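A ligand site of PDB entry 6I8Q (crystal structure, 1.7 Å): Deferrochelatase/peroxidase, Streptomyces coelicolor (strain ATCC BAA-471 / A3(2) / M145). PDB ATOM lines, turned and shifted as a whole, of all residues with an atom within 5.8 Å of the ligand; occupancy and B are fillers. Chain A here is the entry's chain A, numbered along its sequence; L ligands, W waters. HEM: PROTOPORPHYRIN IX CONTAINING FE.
A ring nitrogen (NE2) of His 272 binds an iron atom (FE) of the ligand. The backbone NH (N) of Gly 186 is in hydrogen-bond range of an oxygen (O2A) of the ligand, at 2.6 Å. The backbone NH of Arg 188 lies within hydrogen-bond range of an oxygen (O1A) of the ligand (3.0 Å). The guanidinium group (NE) of Arg 188 lies within salt-bridge range of an oxygen (O2D) of the ligand, at 2.8 Å. NH1 of Arg 288 is in salt-bridge range of O2A of the ligand, 2.9 Å away. The backbone NH (N) of Thr 187 sits at hydrogen-bond distance from an oxygen (O2A) of the ligand (3.3 Å).
O of Arg 188 is in hydrogen-bond range of NH2 of Arg 288 (2.8 Å). NH1 of Arg 188 lies within hydrogen-bond range of NE2 of His 277, 3.4 Å away. The side-chain carboxylate (OD1) of Asp 185 is in salt-bridge range of the guanidinium group (NH1) of Arg 288, 3.1 Å away. The backbone NH (N) of Arg 288 lies within hydrogen-bond range of the side-chain amide oxygen (OD1) of Asn 189 (2.8 Å). O of Phe 243 lies within hydrogen-bond range of N of Val 273 (3.0 Å). O of Phe 183 lies close to OD1 of Asn 179 (3.4 Å). The side-chain amide oxygen of Asn 179 lies within hydrogen-bond range of the backbone NH of Leu 181. N of Leu 307 lies within hydrogen-bond range of O of Ile 224.
Residues that only touch the ligand: Pro 278, Lys 184, Phe 320, His 277, Phe 243, Asn 179, Phe 309, Ala 276, Met 226, Asp 185, Gln 324, Leu 332, Leu 307, Phe 183, Val 273, Leu 181, Arg 245, Ile 336, Leu 327 and Val 323. Hydrophobic or aromatic side chains within 4 Å of the ligand: Leu 181, Phe 183, Met 226, Phe 243, His 272, Val 273, Ala 276, His 277, Pro 278, Leu 307, Phe 309, Phe 320, Val 323, Leu 327, Leu 332 and Ile 336. The nearest printed residue that does not touch the ligand is His 338 (4.03 Å).
Water W1 lies within hydrogen-bond range of an oxygen (O1D) of the ligand (2.8 Å) and the backbone carbonyl oxygen (O) of Arg 188 (3.0 Å). Water W3 bridges the guanidinium group (NH2) of Arg 245 (2.5 Å) and an oxygen (O1A) of the ligand (2.9 Å).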
ATOM      1  N   ASN A 179     -14.733 -13.501  -5.319  1.00  0.00           N
ATOM      2  CA  ASN A 179     -14.742 -12.410  -4.372  1.00  0.00           C
ATOM      3  C   ASN A 179     -13.402 -11.658  -4.431  1.00  0.00           C
ATOM      4  O   ASN A 179     -12.540 -11.971  -5.251  1.00  0.00           O
ATOM      5  CB  ASN A 179     -15.074 -12.926  -2.960  1.00  0.00           C
ATOM      6  CG  ASN A 179     -14.198 -14.089  -2.537  1.00  0.00           C
ATOM      7  OD1 ASN A 179     -12.984 -14.068  -2.717  1.00  0.00           O
ATOM      8  ND2 ASN A 179     -14.803 -15.127  -1.970  1.00  0.00           N
ATOM      9  N   LEU A 181     -10.975 -11.771  -2.453  1.00  0.00           N
ATOM     10  CA  LEU A 181      -9.831 -12.598  -2.094  1.00  0.00           C
ATOM     11  C   LEU A 181      -9.359 -13.465  -3.245  1.00  0.00           C
ATOM     12  O   LEU A 181      -8.383 -14.212  -3.085  1.00  0.00           O
ATOM     13  CB  LEU A 181     -10.162 -13.491  -0.889  1.00  0.00           C
ATOM     14  CG  LEU A 181     -10.655 -12.787   0.365  1.00  0.00           C
ATOM     15  CD1 LEU A 181     -10.876 -13.758   1.519  1.00  0.00           C
ATOM     16  CD2 LEU A 181      -9.685 -11.684   0.761  1.00  0.00           C
ATOM     17  N   PHE A 183     -11.017 -15.971  -4.824  1.00  0.00           N
ATOM     18  CA  PHE A 183     -11.570 -17.313  -4.901  1.00  0.00           C
ATOM     19  C   PHE A 183     -12.992 -17.266  -5.439  1.00  0.00           C
ATOM     20  O   PHE A 183     -13.747 -16.325  -5.183  1.00  0.00           O
ATOM     21  CB  PHE A 183     -11.574 -17.993  -3.519  1.00  0.00           C
ATOM     22  CG  PHE A 183     -10.247 -18.566  -3.121  1.00  0.00           C
ATOM     23  CD1 PHE A 183      -9.205 -17.742  -2.716  1.00  0.00           C
ATOM     24  CD2 PHE A 183     -10.036 -19.935  -3.145  1.00  0.00           C
ATOM     25  CE1 PHE A 183      -7.988 -18.295  -2.342  1.00  0.00           C
ATOM     26  CE2 PHE A 183      -8.815 -20.490  -2.758  1.00  0.00           C
ATOM     27  CZ  PHE A 183      -7.784 -19.668  -2.388  1.00  0.00           C
ATOM     28  N   LYS A 184     -13.352 -18.298  -6.208  1.00  0.00           N
ATOM     29  CA  LYS A 184     -14.746 -18.467  -6.634  1.00  0.00           C
ATOM     30  C   LYS A 184     -15.653 -18.571  -5.411  1.00  0.00           C
ATOM     31  O   LYS A 184     -15.321 -19.214  -4.422  1.00  0.00           O
ATOM     32  CB  LYS A 184     -14.901 -19.726  -7.495  1.00  0.00           C
ATOM     33  CG  LYS A 184     -14.245 -19.670  -8.858  1.00  0.00           C
ATOM     34  CD  LYS A 184     -14.370 -21.042  -9.542  1.00  0.00           C
ATOM     35  CE  LYS A 184     -13.808 -21.002 -10.961  1.00  0.00           C
ATOM     36  NZ  LYS A 184     -13.795 -22.369 -11.544  1.00  0.00           N
ATOM     37  N   ASP A 185     -16.808 -17.924  -5.494  1.00  0.00           N
ATOM     38  CA  ASP A 185     -17.743 -17.842  -4.371  1.00  0.00           C
ATOM     39  C   ASP A 185     -19.130 -18.190  -4.899  1.00  0.00           C
ATOM     40  O   ASP A 185     -19.673 -17.428  -5.705  1.00  0.00           O
ATOM     41  CB  ASP A 185     -17.753 -16.449  -3.756  1.00  0.00           C
ATOM     42  CG  ASP A 185     -17.980 -16.437  -2.236  1.00  0.00           C
ATOM     43  OD1 ASP A 185     -18.719 -17.288  -1.670  1.00  0.00           O
ATOM     44  OD2 ASP A 185     -17.383 -15.533  -1.599  1.00  0.00           O
ATOM     45  N   GLY A 186     -19.706 -19.309  -4.440  1.00  0.00           N
ATOM     46  CA  GLY A 186     -21.046 -19.665  -4.886  1.00  0.00           C
ATOM     47  C   GLY A 186     -21.219 -21.069  -5.441  1.00  0.00           C
ATOM     48  O   GLY A 186     -22.339 -21.464  -5.771  1.00  0.00           O
ATOM     49  N   THR A 187     -20.127 -21.837  -5.505  1.00  0.00           N
ATOM     50  CA  THR A 187     -20.145 -23.177  -6.098  1.00  0.00           C
ATOM     51  C   THR A 187     -21.217 -24.065  -5.467  1.00  0.00           C
ATOM     52  O   THR A 187     -22.167 -24.488  -6.120  1.00  0.00           O
ATOM     53  CB  THR A 187     -18.757 -23.794  -5.961  1.00  0.00           C
ATOM     54  OG1 THR A 187     -17.789 -22.871  -6.467  1.00  0.00           O
ATOM     55  CG2 THR A 187     -18.649 -25.118  -6.731  1.00  0.00           C
ATOM     56  N   ARG A 188     -21.089 -24.351  -4.168  1.00  0.00           N
ATOM     57  CA  ARG A 188     -22.064 -25.168  -3.461  1.00  0.00           C
ATOM     58  C   ARG A 188     -23.030 -24.227  -2.734  1.00  0.00           C
ATOM     59  O   ARG A 188     -22.936 -23.965  -1.543  1.00  0.00           O
ATOM     60  CB  ARG A 188     -21.374 -26.159  -2.528  1.00  0.00           C
ATOM     61  CG  ARG A 188     -20.688 -27.296  -3.288  1.00  0.00           C
ATOM     62  CD  ARG A 188     -20.253 -28.466  -2.385  1.00  0.00           C
ATOM     63  NE  ARG A 188     -21.016 -28.487  -1.142  1.00  0.00           N
ATOM     64  CZ  ARG A 188     -22.132 -29.185  -0.964  1.00  0.00           C
ATOM     65  NH1 ARG A 188     -22.785 -29.123   0.191  1.00  0.00           N
ATOM     66  NH2 ARG A 188     -22.594 -29.953  -1.935  1.00  0.00           N
ATOM     67  N   ASN A 189     -23.964 -23.699  -3.507  1.00  0.00           N
ATOM     68  CA  ASN A 189     -25.085 -22.930  -2.996  1.00  0.00           C
ATOM     69  C   ASN A 189     -26.369 -23.715  -3.315  1.00  0.00           C
ATOM     70  O   ASN A 189     -26.313 -24.883  -3.713  1.00  0.00           O
ATOM     71  CB  ASN A 189     -25.060 -21.517  -3.585  1.00  0.00           C
ATOM     72  CG  ASN A 189     -25.835 -20.508  -2.750  1.00  0.00           C
ATOM     73  OD1 ASN A 189     -25.877 -20.600  -1.537  1.00  0.00           O
ATOM     74  ND2 ASN A 189     -26.442 -19.540  -3.413  1.00  0.00           N
ATOM     75  N   ILE A 224     -18.878  -7.376   6.146  1.00  0.00           N
ATOM     76  CA  ILE A 224     -17.642  -8.036   6.559  1.00  0.00           C
ATOM     77  C   ILE A 224     -16.462  -7.329   5.910  1.00  0.00           C
ATOM     78  O   ILE A 224     -16.363  -7.301   4.671  1.00  0.00           O
ATOM     79  CB  ILE A 224     -17.655  -9.528   6.212  1.00  0.00           C
ATOM     80  CG1 ILE A 224     -18.917 -10.144   6.795  1.00  0.00           C
ATOM     81  CG2 ILE A 224     -16.414 -10.236   6.759  1.00  0.00           C
ATOM     82  CD1 ILE A 224     -19.126 -11.556   6.398  1.00  0.00           C
ATOM     83  N   MET A 226     -12.553  -7.066   4.887  1.00  0.00           N
ATOM     84  CA  MET A 226     -11.450  -7.954   4.536  1.00  0.00           C
ATOM     85  C   MET A 226     -10.129  -7.242   4.804  1.00  0.00           C
ATOM     86  O   MET A 226      -9.924  -6.109   4.369  1.00  0.00           O
ATOM     87  CB  MET A 226     -11.525  -8.375   3.072  1.00  0.00           C
ATOM     88  CG  MET A 226     -12.702  -9.285   2.742  1.00  0.00           C
ATOM     89  SD  MET A 226     -12.931  -9.342   0.935  1.00  0.00           S
ATOM     90  CE  MET A 226     -14.009 -10.751   0.797  1.00  0.00           C
ATOM     91  N   PHE A 243      -9.247 -22.090   2.785  1.00  0.00           N
ATOM     92  CA  PHE A 243     -10.568 -22.420   2.256  1.00  0.00           C
ATOM     93  C   PHE A 243     -10.812 -23.915   2.118  1.00  0.00           C
ATOM     94  O   PHE A 243     -11.907 -24.379   2.463  1.00  0.00           O
ATOM     95  CB  PHE A 243     -10.748 -21.733   0.892  1.00  0.00           C
ATOM     96  CG  PHE A 243     -11.073 -20.283   1.021  1.00  0.00           C
ATOM     97  CD1 PHE A 243     -12.274 -19.888   1.603  1.00  0.00           C
ATOM     98  CD2 PHE A 243     -10.171 -19.322   0.623  1.00  0.00           C
ATOM     99  CE1 PHE A 243     -12.570 -18.546   1.769  1.00  0.00           C
ATOM    100  CE2 PHE A 243     -10.458 -17.982   0.785  1.00  0.00           C
ATOM    101  CZ  PHE A 243     -11.665 -17.599   1.353  1.00  0.00           C
ATOM    102  N   ARG A 245     -10.137 -25.280  -1.027  1.00  0.00           N
ATOM    103  CA  ARG A 245     -10.207 -25.395  -2.472  1.00  0.00           C
ATOM    104  C   ARG A 245      -8.977 -24.716  -3.051  1.00  0.00           C
ATOM    105  O   ARG A 245      -8.396 -23.822  -2.426  1.00  0.00           O
ATOM    106  CB  ARG A 245     -11.497 -24.743  -3.019  1.00  0.00           C
ATOM    107  CG  ARG A 245     -12.797 -25.491  -2.667  1.00  0.00           C
ATOM    108  CD  ARG A 245     -14.008 -24.745  -3.203  1.00  0.00           C
ATOM    109  NE  ARG A 245     -15.282 -25.406  -2.906  1.00  0.00           N
ATOM    110  CZ  ARG A 245     -15.859 -26.332  -3.671  1.00  0.00           C
ATOM    111  NH1 ARG A 245     -15.285 -26.736  -4.796  1.00  0.00           N
ATOM    112  NH2 ARG A 245     -17.031 -26.865  -3.305  1.00  0.00           N
ATOM    113  N   PRO A 262     -16.601 -32.073  -2.412  1.00  0.00           N
ATOM    114  CA  PRO A 262     -15.482 -32.006  -1.471  1.00  0.00           C
ATOM    115  C   PRO A 262     -15.352 -33.277  -0.655  1.00  0.00           C
ATOM    116  O   PRO A 262     -16.336 -33.943  -0.341  1.00  0.00           O
ATOM    117  CB  PRO A 262     -15.823 -30.798  -0.589  1.00  0.00           C
ATOM    118  CG  PRO A 262     -17.265 -30.546  -0.810  1.00  0.00           C
ATOM    119  CD  PRO A 262     -17.610 -31.018  -2.170  1.00  0.00           C
ATOM    120  N   HIS A 272     -12.297 -23.285   5.889  1.00  0.00           N
ATOM    121  CA  HIS A 272     -13.594 -22.630   5.820  1.00  0.00           C
ATOM    122  C   HIS A 272     -14.683 -23.557   5.275  1.00  0.00           C
ATOM    123  O   HIS A 272     -15.773 -23.662   5.852  1.00  0.00           O
ATOM    124  CB  HIS A 272     -13.493 -21.372   4.971  1.00  0.00           C
ATOM    125  CG  HIS A 272     -14.758 -20.580   4.911  1.00  0.00           C
ATOM    126  ND1 HIS A 272     -15.211 -19.830   5.973  1.00  0.00           N
ATOM    127  CD2 HIS A 272     -15.677 -20.438   3.917  1.00  0.00           C
ATOM    128  CE1 HIS A 272     -16.350 -19.243   5.633  1.00  0.00           C
ATOM    129  NE2 HIS A 272     -16.648 -19.597   4.401  1.00  0.00           N
ATOM    130  N   VAL A 273     -14.409 -24.252   4.162  1.00  0.00           N
ATOM    131  CA  VAL A 273     -15.414 -25.115   3.555  1.00  0.00           C
ATOM    132  C   VAL A 273     -15.718 -26.288   4.462  1.00  0.00           C
ATOM    133  O   VAL A 273     -16.875 -26.729   4.567  1.00  0.00           O
ATOM    134  CB  VAL A 273     -14.940 -25.589   2.175  1.00  0.00           C
ATOM    135  CG1 VAL A 273     -15.730 -26.810   1.731  1.00  0.00           C
ATOM    136  CG2 VAL A 273     -15.068 -24.481   1.165  1.00  0.00           C
ATOM    137  N   ALA A 276     -18.020 -24.937   7.248  1.00  0.00           N
ATOM    138  CA  ALA A 276     -19.299 -24.388   6.780  1.00  0.00           C
ATOM    139  C   ALA A 276     -20.201 -25.430   6.141  1.00  0.00           C
ATOM    140  O   ALA A 276     -21.402 -25.171   5.976  1.00  0.00           O
ATOM    141  CB  ALA A 276     -19.050 -23.255   5.781  1.00  0.00           C
ATOM    142  N   HIS A 277     -19.669 -26.586   5.804  1.00  0.00           N
ATOM    143  CA  HIS A 277     -20.390 -27.565   5.008  1.00  0.00           C
ATOM    144  C   HIS A 277     -21.624 -28.057   5.762  1.00  0.00           C
ATOM    145  O   HIS A 277     -21.590 -28.177   6.993  1.00  0.00           O
ATOM    146  CB  HIS A 277     -19.429 -28.721   4.692  1.00  0.00           C
ATOM    147  CG  HIS A 277     -19.895 -29.643   3.605  1.00  0.00           C
ATOM    148  ND1 HIS A 277     -20.779 -30.677   3.825  1.00  0.00           N
ATOM    149  CD2 HIS A 277     -19.557 -29.720   2.297  1.00  0.00           C
ATOM    150  CE1 HIS A 277     -20.987 -31.330   2.705  1.00  0.00           C
ATOM    151  NE2 HIS A 277     -20.250 -30.776   1.757  1.00  0.00           N
ATOM    152  N   PRO A 278     -22.731 -28.348   5.056  1.00  0.00           N
ATOM    153  CA  PRO A 278     -23.906 -28.910   5.760  1.00  0.00           C
ATOM    154  C   PRO A 278     -23.567 -30.118   6.612  1.00  0.00           C
ATOM    155  O   PRO A 278     -24.077 -30.256   7.734  1.00  0.00           O
ATOM    156  CB  PRO A 278     -24.855 -29.253   4.605  1.00  0.00           C
ATOM    157  CG  PRO A 278     -24.550 -28.234   3.566  1.00  0.00           C
ATOM    158  CD  PRO A 278     -23.071 -27.908   3.691  1.00  0.00           C
ATOM    159  N   LEU A 286     -27.768 -23.023   3.614  1.00  0.00           N
ATOM    160  CA  LEU A 286     -28.122 -21.621   3.441  1.00  0.00           C
ATOM    161  C   LEU A 286     -28.170 -21.310   1.950  1.00  0.00           C
ATOM    162  O   LEU A 286     -27.580 -22.025   1.142  1.00  0.00           O
ATOM    163  CB  LEU A 286     -27.110 -20.677   4.101  1.00  0.00           C
ATOM    164  CG  LEU A 286     -26.830 -20.959   5.578  1.00  0.00           C
ATOM    165  CD1 LEU A 286     -25.680 -20.081   6.069  1.00  0.00           C
ATOM    166  CD2 LEU A 286     -28.093 -20.726   6.402  1.00  0.00           C
ATOM    167  N   ARG A 288     -26.813 -18.382  -0.088  1.00  0.00           N
ATOM    168  CA  ARG A 288     -25.949 -17.209  -0.060  1.00  0.00           C
ATOM    169  C   ARG A 288     -26.179 -16.345  -1.288  1.00  0.00           C
ATOM    170  O   ARG A 288     -26.273 -16.858  -2.408  1.00  0.00           O
ATOM    171  CB  ARG A 288     -24.480 -17.633   0.019  1.00  0.00           C
ATOM    172  CG  ARG A 288     -24.073 -18.165   1.403  1.00  0.00           C
ATOM    173  CD  ARG A 288     -22.698 -18.789   1.400  1.00  0.00           C
ATOM    174  NE  ARG A 288     -22.655 -19.997   0.577  1.00  0.00           N
ATOM    175  CZ  ARG A 288     -21.706 -20.281  -0.317  1.00  0.00           C
ATOM    176  NH1 ARG A 288     -20.685 -19.436  -0.521  1.00  0.00           N
ATOM    177  NH2 ARG A 288     -21.792 -21.414  -1.010  1.00  0.00           N
ATOM    178  N   LEU A 307     -16.983  -7.703   1.938  1.00  0.00           N
ATOM    179  CA  LEU A 307     -18.065  -8.520   1.435  1.00  0.00           C
ATOM    180  C   LEU A 307     -19.331  -8.188   2.206  1.00  0.00           C
ATOM    181  O   LEU A 307     -19.324  -8.204   3.444  1.00  0.00           O
ATOM    182  CB  LEU A 307     -17.718 -10.010   1.561  1.00  0.00           C
ATOM    183  CG  LEU A 307     -18.574 -10.979   0.733  1.00  0.00           C
ATOM    184  CD1 LEU A 307     -17.742 -12.190   0.299  1.00  0.00           C
ATOM    185  CD2 LEU A 307     -19.788 -11.412   1.526  1.00  0.00           C
ATOM    186  N   PHE A 309     -22.440  -9.737   3.062  1.00  0.00           N
ATOM    187  CA  PHE A 309     -22.916 -11.114   3.077  1.00  0.00           C
ATOM    188  C   PHE A 309     -24.421 -11.158   3.317  1.00  0.00           C
ATOM    189  O   PHE A 309     -24.927 -10.548   4.272  1.00  0.00           O
ATOM    190  CB  PHE A 309     -22.140 -11.880   4.155  1.00  0.00           C
ATOM    191  CG  PHE A 309     -22.553 -13.328   4.298  1.00  0.00           C
ATOM    192  CD1 PHE A 309     -23.571 -13.686   5.177  1.00  0.00           C
ATOM    193  CD2 PHE A 309     -21.900 -14.327   3.575  1.00  0.00           C
ATOM    194  CE1 PHE A 309     -23.967 -15.015   5.323  1.00  0.00           C
ATOM    195  CE2 PHE A 309     -22.281 -15.665   3.707  1.00  0.00           C
ATOM    196  CZ  PHE A 309     -23.319 -16.012   4.587  1.00  0.00           C
ATOM    197  N   PHE A 320     -28.368 -19.657   9.731  1.00  0.00           N
ATOM    198  CA  PHE A 320     -27.160 -18.864   9.940  1.00  0.00           C
ATOM    199  C   PHE A 320     -26.522 -19.122  11.300  1.00  0.00           C
ATOM    200  O   PHE A 320     -25.280 -19.188  11.413  1.00  0.00           O
ATOM    201  CB  PHE A 320     -27.500 -17.378   9.774  1.00  0.00           C
ATOM    202  CG  PHE A 320     -26.329 -16.474  10.017  1.00  0.00           C
ATOM    203  CD1 PHE A 320     -25.386 -16.260   9.029  1.00  0.00           C
ATOM    204  CD2 PHE A 320     -26.167 -15.860  11.242  1.00  0.00           C
ATOM    205  CE1 PHE A 320     -24.283 -15.437   9.258  1.00  0.00           C
ATOM    206  CE2 PHE A 320     -25.084 -15.027  11.471  1.00  0.00           C
ATOM    207  CZ  PHE A 320     -24.135 -14.820  10.473  1.00  0.00           C
ATOM    208  N   VAL A 323     -24.298 -22.460  11.660  1.00  0.00           N
ATOM    209  CA  VAL A 323     -23.125 -22.402  10.798  1.00  0.00           C
ATOM    210  C   VAL A 323     -22.139 -21.346  11.295  1.00  0.00           C
ATOM    211  O   VAL A 323     -20.935 -21.611  11.437  1.00  0.00           O
ATOM    212  CB  VAL A 323     -23.532 -22.150   9.331  1.00  0.00           C
ATOM    213  CG1 VAL A 323     -22.307 -22.139   8.418  1.00  0.00           C
ATOM    214  CG2 VAL A 323     -24.552 -23.222   8.835  1.00  0.00           C
ATOM    215  N   GLN A 324     -22.618 -20.139  11.608  1.00  0.00           N
ATOM    216  CA  GLN A 324     -21.691 -19.117  12.103  1.00  0.00           C
ATOM    217  C   GLN A 324     -21.095 -19.511  13.457  1.00  0.00           C
ATOM    218  O   GLN A 324     -19.943 -19.161  13.742  1.00  0.00           O
ATOM    219  CB  GLN A 324     -22.375 -17.754  12.171  1.00  0.00           C
ATOM    220  CG  GLN A 324     -21.529 -16.655  12.842  1.00  0.00           C
ATOM    221  CD  GLN A 324     -20.333 -16.149  11.997  1.00  0.00           C
ATOM    222  OE1 GLN A 324     -20.321 -16.268  10.779  1.00  0.00           O
ATOM    223  NE2 GLN A 324     -19.356 -15.560  12.664  1.00  0.00           N
ATOM    224  N   LEU A 327     -18.191 -21.503  12.785  1.00  0.00           N
ATOM    225  CA  LEU A 327     -17.063 -20.760  12.223  1.00  0.00           C
ATOM    226  C   LEU A 327     -16.172 -20.106  13.296  1.00  0.00           C
ATOM    227  O   LEU A 327     -15.315 -19.287  12.951  1.00  0.00           O
ATOM    228  CB  LEU A 327     -17.574 -19.706  11.230  1.00  0.00           C
ATOM    229  CG  LEU A 327     -18.190 -20.204   9.925  1.00  0.00           C
ATOM    230  CD1 LEU A 327     -18.345 -19.063   8.914  1.00  0.00           C
ATOM    231  CD2 LEU A 327     -17.372 -21.377   9.330  1.00  0.00           C
ATOM    232  N   LEU A 332     -10.311 -18.501   8.274  1.00  0.00           N
ATOM    233  CA  LEU A 332     -10.631 -17.255   7.601  1.00  0.00           C
ATOM    234  C   LEU A 332     -10.741 -16.077   8.559  1.00  0.00           C
ATOM    235  O   LEU A 332     -10.571 -14.932   8.143  1.00  0.00           O
ATOM    236  CB  LEU A 332     -11.942 -17.414   6.831  1.00  0.00           C
ATOM    237  CG  LEU A 332     -12.376 -16.213   5.984  1.00  0.00           C
ATOM    238  CD1 LEU A 332     -11.247 -15.847   5.051  1.00  0.00           C
ATOM    239  CD2 LEU A 332     -13.639 -16.503   5.220  1.00  0.00           C
ATOM    240  N   ILE A 336     -10.749 -11.394   8.221  1.00  0.00           N
ATOM    241  CA  ILE A 336     -12.045 -10.727   8.086  1.00  0.00           C
ATOM    242  C   ILE A 336     -12.487 -10.214   9.448  1.00  0.00           C
ATOM    243  O   ILE A 336     -11.993 -10.644  10.492  1.00  0.00           O
ATOM    244  CB  ILE A 336     -13.135 -11.666   7.510  1.00  0.00           C
ATOM    245  CG1 ILE A 336     -13.379 -12.858   8.448  1.00  0.00           C
ATOM    246  CG2 ILE A 336     -12.786 -12.138   6.100  1.00  0.00           C
ATOM    247  CD1 ILE A 336     -14.763 -13.436   8.327  1.00  0.00           C
ATOM    248  N   HIS A 338     -16.462  -8.862  11.118  1.00  0.00           N
ATOM    249  CA  HIS A 338     -17.870  -8.487  10.918  1.00  0.00           C
ATOM    250  C   HIS A 338     -18.104  -7.134  11.580  1.00  0.00           C
ATOM    251  O   HIS A 338     -17.912  -6.984  12.793  1.00  0.00           O
ATOM    252  CB  HIS A 338     -18.819  -9.536  11.505  1.00  0.00           C
ATOM    253  CG  HIS A 338     -18.734 -10.864  10.831  1.00  0.00           C
ATOM    254  ND1 HIS A 338     -19.824 -11.493  10.259  1.00  0.00           N
ATOM    255  CD2 HIS A 338     -17.669 -11.677  10.598  1.00  0.00           C
ATOM    256  CE1 HIS A 338     -19.436 -12.638   9.728  1.00  0.00           C
ATOM    257  NE2 HIS A 338     -18.147 -12.777   9.921  1.00  0.00           N
HETATM  258  CHA HEM L   1     -18.265 -21.647   0.818  1.00  0.00           C
HETATM  259  CHB HEM L   1     -15.738 -17.501   0.933  1.00  0.00           C
HETATM  260  CHC HEM L   1     -18.199 -15.871   4.772  1.00  0.00           C
HETATM  261  CHD HEM L   1     -20.839 -19.956   4.572  1.00  0.00           C
HETATM  262  C1A HEM L   1     -17.349 -20.677   0.528  1.00  0.00           C
HETATM  263  C2A HEM L   1     -16.366 -20.715  -0.528  1.00  0.00           C
HETATM  264  C3A HEM L   1     -15.680 -19.572  -0.481  1.00  0.00           C
HETATM  265  C4A HEM L   1     -16.203 -18.755   0.596  1.00  0.00           C
HETATM  266  CMA HEM L   1     -14.500 -19.138  -1.383  1.00  0.00           C
HETATM  267  CAA HEM L   1     -16.161 -21.924  -1.474  1.00  0.00           C
HETATM  268  CBA HEM L   1     -17.057 -21.916  -2.709  1.00  0.00           C
HETATM  269  CGA HEM L   1     -18.537 -22.017  -2.432  1.00  0.00           C
HETATM  270  O1A HEM L   1     -19.063 -23.142  -2.249  1.00  0.00           O
HETATM  271  O2A HEM L   1     -19.199 -20.961  -2.434  1.00  0.00           O
HETATM  272  C1B HEM L   1     -16.198 -16.688   1.946  1.00  0.00           C
HETATM  273  C2B HEM L   1     -15.735 -15.351   2.242  1.00  0.00           C
HETATM  274  C3B HEM L   1     -16.390 -14.901   3.324  1.00  0.00           C
HETATM  275  C4B HEM L   1     -17.322 -15.928   3.722  1.00  0.00           C
HETATM  276  CMB HEM L   1     -14.624 -14.633   1.436  1.00  0.00           C
HETATM  277  CAB HEM L   1     -16.277 -13.522   4.035  1.00  0.00           C
HETATM  278  CBB HEM L   1     -15.637 -12.495   3.448  1.00  0.00           C
HETATM  279  C1C HEM L   1     -19.135 -16.830   5.061  1.00  0.00           C
HETATM  280  C2C HEM L   1     -20.098 -16.813   6.154  1.00  0.00           C
HETATM  281  C3C HEM L   1     -20.812 -17.942   6.079  1.00  0.00           C
HETATM  282  C4C HEM L   1     -20.339 -18.719   4.963  1.00  0.00           C
HETATM  283  CMC HEM L   1     -20.207 -15.632   7.150  1.00  0.00           C
HETATM  284  CAC HEM L   1     -21.971 -18.452   6.980  1.00  0.00           C
HETATM  285  CBC HEM L   1     -22.276 -17.834   8.129  1.00  0.00           C
HETATM  286  C1D HEM L   1     -20.387 -20.735   3.522  1.00  0.00           C
HETATM  287  C2D HEM L   1     -20.985 -21.974   3.093  1.00  0.00           C
HETATM  288  C3D HEM L   1     -20.277 -22.459   2.058  1.00  0.00           C
HETATM  289  C4D HEM L   1     -19.210 -21.529   1.792  1.00  0.00           C
HETATM  290  CMD HEM L   1     -22.229 -22.621   3.747  1.00  0.00           C
HETATM  291  CAD HEM L   1     -20.548 -23.756   1.279  1.00  0.00           C
HETATM  292  CBD HEM L   1     -19.769 -24.918   1.864  1.00  0.00           C
HETATM  293  CGD HEM L   1     -20.218 -26.205   1.221  1.00  0.00           C
HETATM  294  O1D HEM L   1     -21.391 -26.578   1.482  1.00  0.00           O
HETATM  295  O2D HEM L   1     -19.428 -26.836   0.477  1.00  0.00           O
HETATM  296  NA  HEM L   1     -17.230 -19.461   1.193  1.00  0.00           N
HETATM  297  NB  HEM L   1     -17.156 -17.009   2.864  1.00  0.00           N
HETATM  298  NC  HEM L   1     -19.292 -18.024   4.366  1.00  0.00           N
HETATM  299  ND  HEM L   1     -19.314 -20.492   2.700  1.00  0.00           N
HETATM  300 FE   HEM L   1     -18.187 -18.798   2.869  1.00  0.00          FE
HETATM  301  O   HOH W   1     -23.851 -25.489   0.896  1.00  0.00           O
HETATM  302  O   HOH W   2     -24.204 -24.761   5.399  1.00  0.00           O
HETATM  303  O   HOH W   3     -17.518 -25.380  -1.293  1.00  0.00           O
HETATM  304  O   HOH W   4     -25.141 -24.224   2.871  1.00  0.00           O
